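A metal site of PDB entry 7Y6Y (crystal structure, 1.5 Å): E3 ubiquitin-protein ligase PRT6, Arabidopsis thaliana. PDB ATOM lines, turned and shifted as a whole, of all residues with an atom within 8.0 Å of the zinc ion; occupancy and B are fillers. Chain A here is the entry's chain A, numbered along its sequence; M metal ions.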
ATOM      1  N   ARG A  21      22.887  -4.610  16.870  1.00  0.00           N
ATOM      2  CA  ARG A  21      22.296  -5.805  17.427  1.00  0.00           C
ATOM      3  C   ARG A  21      23.430  -6.596  18.075  1.00  0.00           C
ATOM      4  O   ARG A  21      24.499  -6.742  17.489  1.00  0.00           O
ATOM      5  CB  ARG A  21      21.639  -6.656  16.334  1.00  0.00           C
ATOM      6  CG  ARG A  21      21.126  -7.982  16.849  1.00  0.00           C
ATOM      7  CD  ARG A  21      20.132  -8.605  15.916  1.00  0.00           C
ATOM      8  NE  ARG A  21      19.515  -9.719  16.622  1.00  0.00           N
ATOM      9  CZ  ARG A  21      18.964 -10.760  16.021  1.00  0.00           C
ATOM     10  NH1 ARG A  21      18.971 -10.812  14.689  1.00  0.00           N
ATOM     11  NH2 ARG A  21      18.440 -11.725  16.752  1.00  0.00           N
ATOM     12  N   CYS A  22      23.196  -7.151  19.262  1.00  0.00           N
ATOM     13  CA  CYS A  22      24.148  -8.105  19.822  1.00  0.00           C
ATOM     14  C   CYS A  22      23.376  -9.317  20.266  1.00  0.00           C
ATOM     15  O   CYS A  22      22.607  -9.261  21.228  1.00  0.00           O
ATOM     16  CB  CYS A  22      24.948  -7.541  21.004  1.00  0.00           C
ATOM     17  SG  CYS A  22      26.176  -8.806  21.497  1.00  0.00           S
ATOM     18  N   ARG A  23      23.550 -10.430  19.536  1.00  0.00           N
ATOM     19  CA  ARG A  23      22.749 -11.621  19.820  1.00  0.00           C
ATOM     20  C   ARG A  23      23.133 -12.268  21.135  1.00  0.00           C
ATOM     21  O   ARG A  23      22.348 -13.061  21.672  1.00  0.00           O
ATOM     22  CB  ARG A  23      22.904 -12.593  18.660  1.00  0.00           C
ATOM     23  CG  ARG A  23      22.265 -12.090  17.410  1.00  0.00           C
ATOM     24  CD  ARG A  23      22.804 -12.771  16.215  1.00  0.00           C
ATOM     25  NE  ARG A  23      22.407 -12.163  14.954  1.00  0.00           N
ATOM     26  CZ  ARG A  23      23.016 -11.117  14.401  1.00  0.00           C
ATOM     27  NH1 ARG A  23      24.043 -10.555  15.029  1.00  0.00           N
ATOM     28  NH2 ARG A  23      22.632 -10.651  13.226  1.00  0.00           N
ATOM     29  N   THR A  24      24.347 -11.990  21.626  1.00  0.00           N
ATOM     30  CA  THR A  24      24.788 -12.512  22.915  1.00  0.00           C
ATOM     31  C   THR A  24      24.120 -11.774  24.075  1.00  0.00           C
ATOM     32  O   THR A  24      23.789 -12.401  25.103  1.00  0.00           O
ATOM     33  CB  THR A  24      26.311 -12.373  22.957  1.00  0.00           C
ATOM     34  OG1 THR A  24      26.889 -12.932  21.749  1.00  0.00           O
ATOM     35  CG2 THR A  24      26.884 -13.094  24.151  1.00  0.00           C
ATOM     36  N   CYS A  25      23.834 -10.485  23.903  1.00  0.00           N
ATOM     37  CA  CYS A  25      23.371  -9.643  24.995  1.00  0.00           C
ATOM     38  C   CYS A  25      21.879  -9.353  24.969  1.00  0.00           C
ATOM     39  O   CYS A  25      21.297  -8.989  26.009  1.00  0.00           O
ATOM     40  CB  CYS A  25      24.118  -8.294  24.989  1.00  0.00           C
ATOM     41  SG  CYS A  25      25.842  -8.344  25.445  1.00  0.00           S
ATOM     42  N   GLU A  26      21.222  -9.496  23.823  1.00  0.00           N
ATOM     43  CA  GLU A  26      19.839  -9.080  23.713  1.00  0.00           C
ATOM     44  C   GLU A  26      18.931  -9.967  24.574  1.00  0.00           C
ATOM     45  O   GLU A  26      19.179 -11.168  24.724  1.00  0.00           O
ATOM     46  CB  GLU A  26      19.379  -9.160  22.252  1.00  0.00           C
ATOM     47  CG  GLU A  26      19.409 -10.563  21.690  1.00  0.00           C
ATOM     48  CD  GLU A  26      19.140 -10.652  20.197  1.00  0.00           C
ATOM     49  OE1 GLU A  26      19.421  -9.663  19.505  1.00  0.00           O
ATOM     50  OE2 GLU A  26      18.674 -11.724  19.733  1.00  0.00           O
ATOM     51  N   ILE A  33      21.107  -1.600  20.765  1.00  0.00           N
ATOM     52  CA  ILE A  33      21.766  -0.541  21.506  1.00  0.00           C
ATOM     53  C   ILE A  33      22.426   0.417  20.533  1.00  0.00           C
ATOM     54  O   ILE A  33      22.867   0.052  19.436  1.00  0.00           O
ATOM     55  CB  ILE A  33      22.771  -1.032  22.554  1.00  0.00           C
ATOM     56  CG1 ILE A  33      23.917  -1.841  21.957  1.00  0.00           C
ATOM     57  CG2 ILE A  33      21.998  -1.817  23.646  1.00  0.00           C
ATOM     58  CD1 ILE A  33      24.970  -2.052  23.061  1.00  0.00           C
ATOM     59  N   PHE A  38      27.351   0.741  22.493  1.00  0.00           N
ATOM     60  CA  PHE A  38      28.115  -0.417  22.054  1.00  0.00           C
ATOM     61  C   PHE A  38      29.604  -0.195  22.256  1.00  0.00           C
ATOM     62  O   PHE A  38      30.326  -1.064  22.757  1.00  0.00           O
ATOM     63  CB  PHE A  38      27.819  -0.742  20.575  1.00  0.00           C
ATOM     64  CG  PHE A  38      28.559  -1.949  20.082  1.00  0.00           C
ATOM     65  CD1 PHE A  38      28.045  -3.207  20.277  1.00  0.00           C
ATOM     66  CD2 PHE A  38      29.785  -1.811  19.449  1.00  0.00           C
ATOM     67  CE1 PHE A  38      28.748  -4.338  19.834  1.00  0.00           C
ATOM     68  CE2 PHE A  38      30.490  -2.907  18.992  1.00  0.00           C
ATOM     69  CZ  PHE A  38      29.962  -4.175  19.205  1.00  0.00           C
ATOM     70  N   GLY A  41      30.930  -0.539  25.877  1.00  0.00           N
ATOM     71  CA  GLY A  41      30.739  -1.807  26.555  1.00  0.00           C
ATOM     72  C   GLY A  41      31.709  -2.861  26.049  1.00  0.00           C
ATOM     73  O   GLY A  41      32.615  -2.541  25.284  1.00  0.00           O
ATOM     74  N   ASP A  42      31.562  -4.115  26.481  1.00  0.00           N
ATOM     75  CA  ASP A  42      32.487  -5.161  26.039  1.00  0.00           C
ATOM     76  C   ASP A  42      31.690  -6.220  25.292  1.00  0.00           C
ATOM     77  O   ASP A  42      30.918  -6.974  25.915  1.00  0.00           O
ATOM     78  CB  ASP A  42      33.244  -5.772  27.223  1.00  0.00           C
ATOM     79  CG  ASP A  42      34.324  -6.786  26.777  1.00  0.00           C
ATOM     80  OD1 ASP A  42      34.125  -7.468  25.740  1.00  0.00           O
ATOM     81  OD2 ASP A  42      35.374  -6.895  27.445  1.00  0.00           O
ATOM     82  N   HIS A  43      31.864  -6.283  23.965  1.00  0.00           N
ATOM     83  CA  HIS A  43      31.235  -7.307  23.136  1.00  0.00           C
ATOM     84  C   HIS A  43      32.247  -8.072  22.285  1.00  0.00           C
ATOM     85  O   HIS A  43      31.909  -8.602  21.227  1.00  0.00           O
ATOM     86  CB  HIS A  43      30.147  -6.677  22.264  1.00  0.00           C
ATOM     87  CG  HIS A  43      29.170  -5.861  23.042  1.00  0.00           C
ATOM     88  ND1 HIS A  43      28.025  -6.382  23.600  1.00  0.00           N
ATOM     89  CD2 HIS A  43      29.223  -4.566  23.444  1.00  0.00           C
ATOM     90  CE1 HIS A  43      27.388  -5.430  24.268  1.00  0.00           C
ATOM     91  NE2 HIS A  43      28.100  -4.328  24.181  1.00  0.00           N
ATOM     92  N   ASN A  44      33.481  -8.202  22.777  1.00  0.00           N
ATOM     93  CA  ASN A  44      34.577  -8.641  21.901  1.00  0.00           C
ATOM     94  C   ASN A  44      34.288  -9.962  21.195  1.00  0.00           C
ATOM     95  O   ASN A  44      34.406 -10.068  19.969  1.00  0.00           O
ATOM     96  CB  ASN A  44      35.861  -8.742  22.733  1.00  0.00           C
ATOM     97  CG  ASN A  44      36.470  -7.374  23.037  1.00  0.00           C
ATOM     98  OD1 ASN A  44      37.054  -7.166  24.110  1.00  0.00           O
ATOM     99  ND2 ASN A  44      36.329  -6.426  22.092  1.00  0.00           N
ATOM    100  N   SER A  45      33.931 -10.997  21.950  1.00  0.00           N
ATOM    101  CA  SER A  45      33.660 -12.296  21.357  1.00  0.00           C
ATOM    102  C   SER A  45      32.182 -12.504  21.044  1.00  0.00           C
ATOM    103  O   SER A  45      31.770 -13.636  20.812  1.00  0.00           O
ATOM    104  CB  SER A  45      34.142 -13.408  22.282  1.00  0.00           C
ATOM    105  OG  SER A  45      33.311 -13.474  23.433  1.00  0.00           O
ATOM    106  N   HIS A  46      31.376 -11.441  21.043  1.00  0.00           N
ATOM    107  CA  HIS A  46      29.937 -11.566  20.912  1.00  0.00           C
ATOM    108  C   HIS A  46      29.510 -11.616  19.457  1.00  0.00           C
ATOM    109  O   HIS A  46      30.252 -11.193  18.565  1.00  0.00           O
ATOM    110  CB  HIS A  46      29.246 -10.383  21.596  1.00  0.00           C
ATOM    111  CG  HIS A  46      29.419 -10.366  23.069  1.00  0.00           C
ATOM    112  ND1 HIS A  46      28.627  -9.580  23.882  1.00  0.00           N
ATOM    113  CD2 HIS A  46      30.282 -11.010  23.885  1.00  0.00           C
ATOM    114  CE1 HIS A  46      28.981  -9.777  25.150  1.00  0.00           C
ATOM    115  NE2 HIS A  46      30.003 -10.619  25.173  1.00  0.00           N
ATOM    116  N   ASP A  47      28.276 -12.069  19.214  1.00  0.00           N
ATOM    117  CA  ASP A  47      27.761 -12.150  17.848  1.00  0.00           C
ATOM    118  C   ASP A  47      26.926 -10.915  17.532  1.00  0.00           C
ATOM    119  O   ASP A  47      25.696 -10.916  17.562  1.00  0.00           O
ATOM    120  CB  ASP A  47      26.965 -13.422  17.636  1.00  0.00           C
ATOM    121  CG  ASP A  47      26.565 -13.606  16.161  1.00  0.00           C
ATOM    122  OD1 ASP A  47      26.997 -12.772  15.304  1.00  0.00           O
ATOM    123  OD2 ASP A  47      25.778 -14.563  15.921  1.00  0.00           O
ATOM    124  N   TYR A  48      27.626  -9.836  17.220  1.00  0.00           N
ATOM    125  CA  TYR A  48      27.008  -8.526  17.001  1.00  0.00           C
ATOM    126  C   TYR A  48      27.082  -8.146  15.520  1.00  0.00           C
ATOM    127  O   TYR A  48      27.925  -8.641  14.755  1.00  0.00           O
ATOM    128  CB  TYR A  48      27.694  -7.448  17.845  1.00  0.00           C
ATOM    129  CG  TYR A  48      29.167  -7.238  17.558  1.00  0.00           C
ATOM    130  CD1 TYR A  48      29.568  -6.430  16.488  1.00  0.00           C
ATOM    131  CD2 TYR A  48      30.153  -7.828  18.335  1.00  0.00           C
ATOM    132  CE1 TYR A  48      30.902  -6.232  16.217  1.00  0.00           C
ATOM    133  CE2 TYR A  48      31.486  -7.659  18.048  1.00  0.00           C
ATOM    134  CZ  TYR A  48      31.859  -6.852  17.001  1.00  0.00           C
ATOM    135  OH  TYR A  48      33.186  -6.658  16.695  1.00  0.00           O
ATOM    136  N   TRP A  66      17.962  -6.046  27.856  1.00  0.00           N
ATOM    137  CA  TRP A  66      19.375  -6.265  27.576  1.00  0.00           C
ATOM    138  C   TRP A  66      20.047  -6.862  28.814  1.00  0.00           C
ATOM    139  O   TRP A  66      19.744  -6.456  29.948  1.00  0.00           O
ATOM    140  CB  TRP A  66      19.978  -4.912  27.192  1.00  0.00           C
ATOM    141  CG  TRP A  66      21.248  -4.918  26.409  1.00  0.00           C
ATOM    142  CD1 TRP A  66      22.509  -4.760  26.898  1.00  0.00           C
ATOM    143  CD2 TRP A  66      21.374  -5.085  25.003  1.00  0.00           C
ATOM    144  NE1 TRP A  66      23.430  -4.814  25.865  1.00  0.00           N
ATOM    145  CE2 TRP A  66      22.735  -5.009  24.691  1.00  0.00           C
ATOM    146  CE3 TRP A  66      20.452  -5.264  23.965  1.00  0.00           C
ATOM    147  CZ2 TRP A  66      23.208  -5.112  23.382  1.00  0.00           C
ATOM    148  CZ3 TRP A  66      20.890  -5.401  22.717  1.00  0.00           C
ATOM    149  CH2 TRP A  66      22.258  -5.315  22.410  1.00  0.00           C
ATOM    150  N   LYS A  67      20.973  -7.771  28.597  1.00  0.00           N
ATOM    151  CA  LYS A  67      21.625  -8.418  29.706  1.00  0.00           C
ATOM    152  C   LYS A  67      22.597  -7.448  30.380  1.00  0.00           C
ATOM    153  O   LYS A  67      23.313  -6.685  29.691  1.00  0.00           O
ATOM    154  CB  LYS A  67      22.346  -9.692  29.275  1.00  0.00           C
ATOM    155  CG  LYS A  67      21.398 -10.759  28.731  1.00  0.00           C
ATOM    156  CD  LYS A  67      22.191 -11.901  28.079  1.00  0.00           C
ATOM    157  CE  LYS A  67      21.289 -12.848  27.321  1.00  0.00           C
ATOM    158  NZ  LYS A  67      22.049 -13.955  26.651  1.00  0.00           N
ATOM    159  N   ASP A  69      25.499  -7.639  31.761  1.00  0.00           N
ATOM    160  CA  ASP A  69      26.895  -7.698  31.367  1.00  0.00           C
ATOM    161  C   ASP A  69      27.147  -7.002  30.034  1.00  0.00           C
ATOM    162  O   ASP A  69      28.304  -6.745  29.681  1.00  0.00           O
ATOM    163  CB  ASP A  69      27.376  -9.151  31.310  1.00  0.00           C
ATOM    164  CG  ASP A  69      26.476 -10.053  30.466  1.00  0.00           C
ATOM    165  OD1 ASP A  69      25.341 -10.360  30.898  1.00  0.00           O
ATOM    166  OD2 ASP A  69      26.937 -10.503  29.375  1.00  0.00           O
ATOM    167  N   GLY A  70      26.086  -6.686  29.281  1.00  0.00           N
ATOM    168  CA  GLY A  70      26.158  -5.953  28.035  1.00  0.00           C
ATOM    169  C   GLY A  70      25.932  -4.473  28.155  1.00  0.00           C
ATOM    170  O   GLY A  70      25.948  -3.763  27.136  1.00  0.00           O
ATOM    171  N   PHE A  71      25.736  -3.961  29.374  1.00  0.00           N
ATOM    172  CA  PHE A  71      25.588  -2.523  29.588  1.00  0.00           C
ATOM    173  C   PHE A  71      26.914  -1.807  29.398  1.00  0.00           C
ATOM    174  O   PHE A  71      27.986  -2.363  29.639  1.00  0.00           O
ATOM    175  CB  PHE A  71      25.113  -2.226  31.000  1.00  0.00           C
ATOM    176  CG  PHE A  71      23.714  -2.665  31.309  1.00  0.00           C
ATOM    177  CD1 PHE A  71      23.256  -2.588  32.627  1.00  0.00           C
ATOM    178  CD2 PHE A  71      22.860  -3.171  30.342  1.00  0.00           C
ATOM    179  CE1 PHE A  71      21.962  -2.968  32.968  1.00  0.00           C
ATOM    180  CE2 PHE A  71      21.557  -3.538  30.672  1.00  0.00           C
ATOM    181  CZ  PHE A  71      21.111  -3.446  31.979  1.00  0.00           C
HETATM  182 ZN    ZN M   1      27.142  -8.223  23.500  1.00  0.00          ZN
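N of Lys 67 is in hydrogen-bond range of O of Cys 25. SG of Cys 22 sits close to N of Thr 24, 3.7 Å away.
The zinc ion is bound by ND1 of His 43 (2.0 Å), ND1 of His 46 (2.0 Å), SG of Cys 22 (2.3 Å) and SG of Cys 25 (2.3 Å).
Four residues have an atom within 4 Å of the zinc ion: Cys 22, Cys 25, His 43 and His 46.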
